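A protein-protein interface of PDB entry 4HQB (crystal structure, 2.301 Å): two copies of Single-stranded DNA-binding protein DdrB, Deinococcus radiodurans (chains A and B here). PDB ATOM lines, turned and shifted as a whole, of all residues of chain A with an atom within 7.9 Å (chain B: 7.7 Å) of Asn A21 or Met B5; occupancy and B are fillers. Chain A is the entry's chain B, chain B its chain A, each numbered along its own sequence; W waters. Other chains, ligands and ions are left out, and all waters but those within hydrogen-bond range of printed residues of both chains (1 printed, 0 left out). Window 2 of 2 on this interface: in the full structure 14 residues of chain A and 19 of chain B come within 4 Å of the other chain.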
ATOM      1  N   MET A   5      17.916   0.755 -19.493  1.00  0.00           N
ATOM      2  CA  MET A   5      18.805   0.292 -18.426  1.00  0.00           C
ATOM      3  C   MET A   5      20.056   1.175 -18.322  1.00  0.00           C
ATOM      4  O   MET A   5      21.052   0.940 -19.008  1.00  0.00           O
ATOM      5  CB  MET A   5      19.194  -1.173 -18.660  1.00  0.00           C
ATOM      6  CG  MET A   5      19.797  -1.872 -17.458  1.00  0.00           C
ATOM      7  N   LEU A   6      20.002   2.184 -17.455  1.00  0.00           N
ATOM      8  CA  LEU A   6      21.067   3.185 -17.361  1.00  0.00           C
ATOM      9  C   LEU A   6      22.134   2.878 -16.312  1.00  0.00           C
ATOM     10  O   LEU A   6      21.899   2.167 -15.340  1.00  0.00           O
ATOM     11  CB  LEU A   6      20.474   4.572 -17.092  1.00  0.00           C
ATOM     12  CG  LEU A   6      19.584   5.182 -18.180  1.00  0.00           C
ATOM     13  N   GLN A   7      23.314   3.444 -16.503  1.00  0.00           N
ATOM     14  CA  GLN A   7      24.359   3.339 -15.498  1.00  0.00           C
ATOM     15  C   GLN A   7      24.859   4.717 -15.178  1.00  0.00           C
ATOM     16  O   GLN A   7      24.944   5.561 -16.064  1.00  0.00           O
ATOM     17  CB  GLN A   7      25.520   2.475 -15.985  1.00  0.00           C
ATOM     18  CG  GLN A   7      25.306   1.013 -15.729  1.00  0.00           C
ATOM     19  CD  GLN A   7      26.313   0.156 -16.442  1.00  0.00           C
ATOM     20  OE1 GLN A   7      26.733   0.478 -17.555  1.00  0.00           O
ATOM     21  NE2 GLN A   7      26.719  -0.940 -15.807  1.00  0.00           N
ATOM     22  N   ILE A   8      25.178   4.939 -13.909  1.00  0.00           N
ATOM     23  CA  ILE A   8      25.719   6.214 -13.463  1.00  0.00           C
ATOM     24  C   ILE A   8      27.054   5.992 -12.754  1.00  0.00           C
ATOM     25  O   ILE A   8      27.186   5.093 -11.925  1.00  0.00           O
ATOM     26  CB  ILE A   8      24.703   6.981 -12.576  1.00  0.00           C
ATOM     27  CG1 ILE A   8      25.334   8.247 -11.986  1.00  0.00           C
ATOM     28  CG2 ILE A   8      24.136   6.076 -11.482  1.00  0.00           C
ATOM     29  CD1 ILE A   8      24.309   9.288 -11.495  1.00  0.00           C
ATOM     30  N   GLU A   9      28.058   6.785 -13.115  1.00  0.00           N
ATOM     31  CA  GLU A   9      29.368   6.681 -12.478  1.00  0.00           C
ATOM     32  C   GLU A   9      29.418   7.631 -11.310  1.00  0.00           C
ATOM     33  O   GLU A   9      29.102   8.795 -11.469  1.00  0.00           O
ATOM     34  CB  GLU A   9      30.479   7.085 -13.439  1.00  0.00           C
ATOM     35  CG  GLU A   9      30.711   6.190 -14.619  1.00  0.00           C
ATOM     36  CD  GLU A   9      32.150   6.294 -15.095  1.00  0.00           C
ATOM     37  OE1 GLU A   9      32.931   7.036 -14.440  1.00  0.00           O
ATOM     38  OE2 GLU A   9      32.498   5.645 -16.111  1.00  0.00           O
ATOM     39  N   PHE A  10      29.851   7.153 -10.149  1.00  0.00           N
ATOM     40  CA  PHE A  10      29.949   8.001  -8.962  1.00  0.00           C
ATOM     41  C   PHE A  10      31.400   8.074  -8.481  1.00  0.00           C
ATOM     42  O   PHE A  10      32.184   7.154  -8.730  1.00  0.00           O
ATOM     43  CB  PHE A  10      29.127   7.401  -7.826  1.00  0.00           C
ATOM     44  CG  PHE A  10      27.644   7.627  -7.926  1.00  0.00           C
ATOM     45  CD1 PHE A  10      27.091   8.880  -7.665  1.00  0.00           C
ATOM     46  CD2 PHE A  10      26.785   6.568  -8.205  1.00  0.00           C
ATOM     47  CE1 PHE A  10      25.723   9.078  -7.741  1.00  0.00           C
ATOM     48  CE2 PHE A  10      25.406   6.772  -8.264  1.00  0.00           C
ATOM     49  CZ  PHE A  10      24.889   8.032  -8.025  1.00  0.00           C
ATOM     50  N   VAL A  18      33.059   4.451  -8.883  1.00  0.00           N
ATOM     51  CA  VAL A  18      32.098   3.372  -8.785  1.00  0.00           C
ATOM     52  C   VAL A  18      30.934   3.583  -9.756  1.00  0.00           C
ATOM     53  O   VAL A  18      30.437   4.703  -9.908  1.00  0.00           O
ATOM     54  CB  VAL A  18      31.586   3.291  -7.336  1.00  0.00           C
ATOM     55  CG1 VAL A  18      30.499   2.272  -7.196  1.00  0.00           C
ATOM     56  CG2 VAL A  18      32.748   2.978  -6.377  1.00  0.00           C
ATOM     57  N   THR A  19      30.499   2.504 -10.401  1.00  0.00           N
ATOM     58  CA  THR A  19      29.357   2.549 -11.326  1.00  0.00           C
ATOM     59  C   THR A  19      28.171   1.760 -10.777  1.00  0.00           C
ATOM     60  O   THR A  19      28.327   0.639 -10.301  1.00  0.00           O
ATOM     61  CB  THR A  19      29.764   2.039 -12.716  1.00  0.00           C
ATOM     62  OG1 THR A  19      30.602   3.023 -13.336  1.00  0.00           O
ATOM     63  CG2 THR A  19      28.549   1.798 -13.600  1.00  0.00           C
ATOM     64  N   VAL A  20      26.985   2.363 -10.824  1.00  0.00           N
ATOM     65  CA  VAL A  20      25.782   1.777 -10.258  1.00  0.00           C
ATOM     66  C   VAL A  20      24.761   1.563 -11.385  1.00  0.00           C
ATOM     67  O   VAL A  20      24.755   2.312 -12.366  1.00  0.00           O
ATOM     68  CB  VAL A  20      25.197   2.711  -9.158  1.00  0.00           C
ATOM     69  CG1 VAL A  20      23.865   2.203  -8.601  1.00  0.00           C
ATOM     70  CG2 VAL A  20      26.186   2.888  -8.042  1.00  0.00           C
ATOM     71  N   ASN A  21      23.916   0.540 -11.252  1.00  0.00           N
ATOM     72  CA  ASN A  21      22.869   0.285 -12.236  1.00  0.00           C
ATOM     73  C   ASN A  21      21.555   0.957 -11.856  1.00  0.00           C
ATOM     74  O   ASN A  21      21.160   0.966 -10.689  1.00  0.00           O
ATOM     75  CB  ASN A  21      22.644  -1.218 -12.419  1.00  0.00           C
ATOM     76  CG  ASN A  21      23.803  -1.906 -13.113  1.00  0.00           C
ATOM     77  OD1 ASN A  21      24.412  -1.356 -14.029  1.00  0.00           O
ATOM     78  ND2 ASN A  21      24.116  -3.120 -12.673  1.00  0.00           N
ATOM     79  N   VAL A  22      20.894   1.534 -12.852  1.00  0.00           N
ATOM     80  CA  VAL A  22      19.576   2.127 -12.672  1.00  0.00           C
ATOM     81  C   VAL A  22      18.566   1.440 -13.594  1.00  0.00           C
ATOM     82  O   VAL A  22      18.803   1.333 -14.797  1.00  0.00           O
ATOM     83  CB  VAL A  22      19.597   3.617 -13.001  1.00  0.00           C
ATOM     84  CG1 VAL A  22      18.277   4.257 -12.621  1.00  0.00           C
ATOM     85  CG2 VAL A  22      20.765   4.297 -12.290  1.00  0.00           C
ATOM     86  N   GLU A  23      17.449   0.981 -13.028  1.00  0.00           N
ATOM     87  CA  GLU A  23      16.423   0.251 -13.784  1.00  0.00           C
ATOM     88  C   GLU A  23      15.800   1.078 -14.911  1.00  0.00           C
ATOM     89  O   GLU A  23      15.946   0.745 -16.085  1.00  0.00           O
ATOM     90  CB  GLU A  23      15.326  -0.275 -12.850  1.00  0.00           C
ATOM     91  N   HIS A  24      15.101   2.152 -14.552  1.00  0.00           N
ATOM     92  CA  HIS A  24      14.521   3.051 -15.550  1.00  0.00           C
ATOM     93  C   HIS A  24      15.049   4.479 -15.391  1.00  0.00           C
ATOM     94  O   HIS A  24      15.332   4.927 -14.278  1.00  0.00           O
ATOM     95  CB  HIS A  24      12.987   3.040 -15.472  1.00  0.00           C
ATOM     96  N   ARG A  27      13.788   6.734 -12.660  1.00  0.00           N
ATOM     97  CA  ARG A  27      14.257   6.583 -11.287  1.00  0.00           C
ATOM     98  C   ARG A  27      15.670   7.147 -11.061  1.00  0.00           C
ATOM     99  O   ARG A  27      16.258   6.959  -9.997  1.00  0.00           O
ATOM    100  CB  ARG A  27      14.199   5.108 -10.878  1.00  0.00           C
ATOM    101  N   VAL A  31      18.058   7.822  -7.558  1.00  0.00           N
ATOM    102  CA  VAL A  31      19.345   7.173  -7.334  1.00  0.00           C
ATOM    103  C   VAL A  31      20.375   8.226  -6.952  1.00  0.00           C
ATOM    104  O   VAL A  31      21.199   8.000  -6.065  1.00  0.00           O
ATOM    105  CB  VAL A  31      19.804   6.386  -8.582  1.00  0.00           C
ATOM    106  CG1 VAL A  31      21.223   5.843  -8.404  1.00  0.00           C
ATOM    107  CG2 VAL A  31      18.827   5.247  -8.886  1.00  0.00           C
ATOM    108  N   TYR A  35      22.432   8.006  -3.193  1.00  0.00           N
ATOM    109  CA  TYR A  35      23.877   8.039  -2.957  1.00  0.00           C
ATOM    110  C   TYR A  35      24.388   9.440  -2.639  1.00  0.00           C
ATOM    111  O   TYR A  35      25.356   9.598  -1.879  1.00  0.00           O
ATOM    112  CB  TYR A  35      24.634   7.428  -4.146  1.00  0.00           C
ATOM    113  CG  TYR A  35      24.310   5.969  -4.311  1.00  0.00           C
ATOM    114  CD1 TYR A  35      24.937   5.016  -3.520  1.00  0.00           C
ATOM    115  CD2 TYR A  35      23.328   5.545  -5.208  1.00  0.00           C
ATOM    116  CE1 TYR A  35      24.636   3.686  -3.641  1.00  0.00           C
ATOM    117  CE2 TYR A  35      23.012   4.196  -5.334  1.00  0.00           C
ATOM    118  CZ  TYR A  35      23.674   3.276  -4.544  1.00  0.00           C
ATOM    119  OH  TYR A  35      23.395   1.937  -4.644  1.00  0.00           O
ATOM    120  N   MET B   5      24.507  -4.801  -7.756  1.00  0.00           N
ATOM    121  CA  MET B   5      25.664  -5.099  -8.607  1.00  0.00           C
ATOM    122  C   MET B   5      26.467  -3.831  -8.945  1.00  0.00           C
ATOM    123  O   MET B   5      26.041  -2.997  -9.736  1.00  0.00           O
ATOM    124  CB  MET B   5      25.219  -5.816  -9.881  1.00  0.00           C
ATOM    125  CG  MET B   5      26.206  -6.854 -10.398  1.00  0.00           C
ATOM    126  N   LEU B   6      27.636  -3.694  -8.334  1.00  0.00           N
ATOM    127  CA  LEU B   6      28.462  -2.500  -8.481  1.00  0.00           C
ATOM    128  C   LEU B   6      29.728  -2.808  -9.280  1.00  0.00           C
ATOM    129  O   LEU B   6      30.210  -3.938  -9.272  1.00  0.00           O
ATOM    130  CB  LEU B   6      28.892  -1.985  -7.095  1.00  0.00           C
ATOM    131  CG  LEU B   6      27.929  -1.277  -6.141  1.00  0.00           C
ATOM    132  CD1 LEU B   6      27.764   0.153  -6.567  1.00  0.00           C
ATOM    133  CD2 LEU B   6      26.558  -1.956  -6.033  1.00  0.00           C
ATOM    134  N   GLN B   7      30.266  -1.792  -9.950  1.00  0.00           N
ATOM    135  CA  GLN B   7      31.596  -1.868 -10.532  1.00  0.00           C
ATOM    136  C   GLN B   7      32.499  -0.816  -9.907  1.00  0.00           C
ATOM    137  O   GLN B   7      32.060   0.297  -9.632  1.00  0.00           O
ATOM    138  CB  GLN B   7      31.545  -1.645 -12.041  1.00  0.00           C
ATOM    139  CG  GLN B   7      30.913  -2.784 -12.812  1.00  0.00           C
ATOM    140  CD  GLN B   7      30.829  -2.477 -14.297  1.00  0.00           C
ATOM    141  OE1 GLN B   7      30.823  -1.312 -14.698  1.00  0.00           O
ATOM    142  NE2 GLN B   7      30.773  -3.522 -15.122  1.00  0.00           N
ATOM    143  N   ASN B  21      34.047  -6.209 -10.648  1.00  0.00           N
ATOM    144  CA  ASN B  21      32.639  -6.289 -10.300  1.00  0.00           C
ATOM    145  C   ASN B  21      32.409  -6.677  -8.839  1.00  0.00           C
ATOM    146  O   ASN B  21      33.104  -7.530  -8.289  1.00  0.00           O
ATOM    147  CB  ASN B  21      31.920  -7.223 -11.271  1.00  0.00           C
ATOM    148  CG  ASN B  21      31.946  -6.692 -12.685  1.00  0.00           C
ATOM    149  OD1 ASN B  21      30.983  -6.087 -13.141  1.00  0.00           O
ATOM    150  ND2 ASN B  21      33.072  -6.869 -13.370  1.00  0.00           N
ATOM    151  N   VAL B  22      31.453  -6.009  -8.209  1.00  0.00           N
ATOM    152  CA  VAL B  22      31.142  -6.225  -6.802  1.00  0.00           C
ATOM    153  C   VAL B  22      29.701  -6.711  -6.673  1.00  0.00           C
ATOM    154  O   VAL B  22      28.771  -6.003  -7.059  1.00  0.00           O
ATOM    155  CB  VAL B  22      31.307  -4.916  -5.993  1.00  0.00           C
ATOM    156  CG1 VAL B  22      31.150  -5.177  -4.496  1.00  0.00           C
ATOM    157  CG2 VAL B  22      32.660  -4.279  -6.276  1.00  0.00           C
ATOM    158  N   GLU B  23      29.529  -7.912  -6.120  1.00  0.00           N
ATOM    159  CA  GLU B  23      28.224  -8.581  -6.046  1.00  0.00           C
ATOM    160  C   GLU B  23      27.145  -7.760  -5.340  1.00  0.00           C
ATOM    161  O   GLU B  23      26.040  -7.581  -5.868  1.00  0.00           O
ATOM    162  CB  GLU B  23      28.363  -9.944  -5.358  1.00  0.00           C
ATOM    163  N   HIS B  24      27.465  -7.278  -4.142  1.00  0.00           N
ATOM    164  CA  HIS B  24      26.553  -6.424  -3.392  1.00  0.00           C
ATOM    165  C   HIS B  24      27.279  -5.187  -2.875  1.00  0.00           C
ATOM    166  O   HIS B  24      28.458  -5.249  -2.524  1.00  0.00           O
ATOM    167  CB  HIS B  24      25.916  -7.192  -2.230  1.00  0.00           C
ATOM    168  N   GLU B  25      26.562  -4.071  -2.824  1.00  0.00           N
ATOM    169  CA  GLU B  25      27.124  -2.797  -2.388  1.00  0.00           C
ATOM    170  C   GLU B  25      27.798  -2.867  -1.017  1.00  0.00           C
ATOM    171  O   GLU B  25      28.838  -2.240  -0.798  1.00  0.00           O
ATOM    172  CB  GLU B  25      26.040  -1.713  -2.387  1.00  0.00           C
ATOM    173  CG  GLU B  25      26.480  -0.378  -1.792  1.00  0.00           C
ATOM    174  CD  GLU B  25      25.382   0.666  -1.836  1.00  0.00           C
ATOM    175  OE1 GLU B  25      24.470   0.534  -2.685  1.00  0.00           O
ATOM    176  OE2 GLU B  25      25.429   1.613  -1.020  1.00  0.00           O
HETATM  177  O   HOH W   1      23.792  -1.251  -9.125  1.00  0.00           O
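N of Thr A19 sits at hydrogen-bond distance from O of Gln B7, at 2.8 Å.
The side-chain hydroxyl (OH) of Tyr A35 sits at hydrogen-bond distance from the side-chain carboxylate (OE1) of Glu B25, 2.6 Å away.
The backbone carbonyl oxygen of Leu B6 sits at hydrogen-bond distance from the backbone NH of Val B22, at 2.6 Å.
The side-chain amide oxygen of Asn B21 is in hydrogen-bond range of the side-chain amide nitrogen of Gln B7, at 3.2 Å.
The side-chain amide oxygen (OD1) of Asn A21 is in hydrogen-bond range of the side-chain amide nitrogen (NE2) of Gln A7 (2.9 Å).
The backbone NH (N) of Val A20 lies within hydrogen-bond range of the backbone carbonyl oxygen (O) of Ile A8 (3.0 Å).
The backbone carbonyl oxygen of Val A18 lies within hydrogen-bond range of the backbone NH of Phe A10, at 2.5 Å.
Among the printed residues, pairs that only touch across the chains: Val A18 with Gln B7, Val A20 with Leu B6, Asn A21 with Met B5, Val A18 with Leu B6 and Thr A19 with Leu B6.
Asn A21 touches just one residue of chain B: Met B5.
Of chain A, only Asn A21 (3.5 Å) comes within 4 Å of Met B5.
Of the printed residues of chain A, Leu B6 touches Val A18, Thr A19 and Val A20.
Printed residues of chain B within 4 Å of Val A20: Leu B6 (3.5 Å).
Of the 8 printed residues of chain B, 4 touch a printed residue of chain A.
Printed residues of chain B that touch a printed residue of chain A: Met B5, Leu B6, Gln B7 and Glu B25.
Hydrophobic or aromatic side chains of chain B that line the printed part of chain A: Leu B6.
Printed residues of chain A that touch a printed residue of chain B: Val A18, Thr A19, Val A20, Asn A21 and Tyr A35.
Among the printed residues, 7 pairs touch across the chains.
Among the printed residues, no Asp or Glu carboxylate lies within 4 Å of a Lys or Arg side-chain nitrogen of the other chain.
Asn A21 touches Met B5, but with the chains exchanged Met A5 does not touch Asn B21 (12.7 Å).
Positions printed for both chains: 5, 6, 7, 21, 22, 23 and 24.
Of the 7 pairs that touch across the chains among the printed residues, none has its exchanged pair printed and touching as well.
Water W1 bridges the backbone NH of Asn A21 (2.8 Å) and the backbone carbonyl oxygen of Met B5 (2.9 Å).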
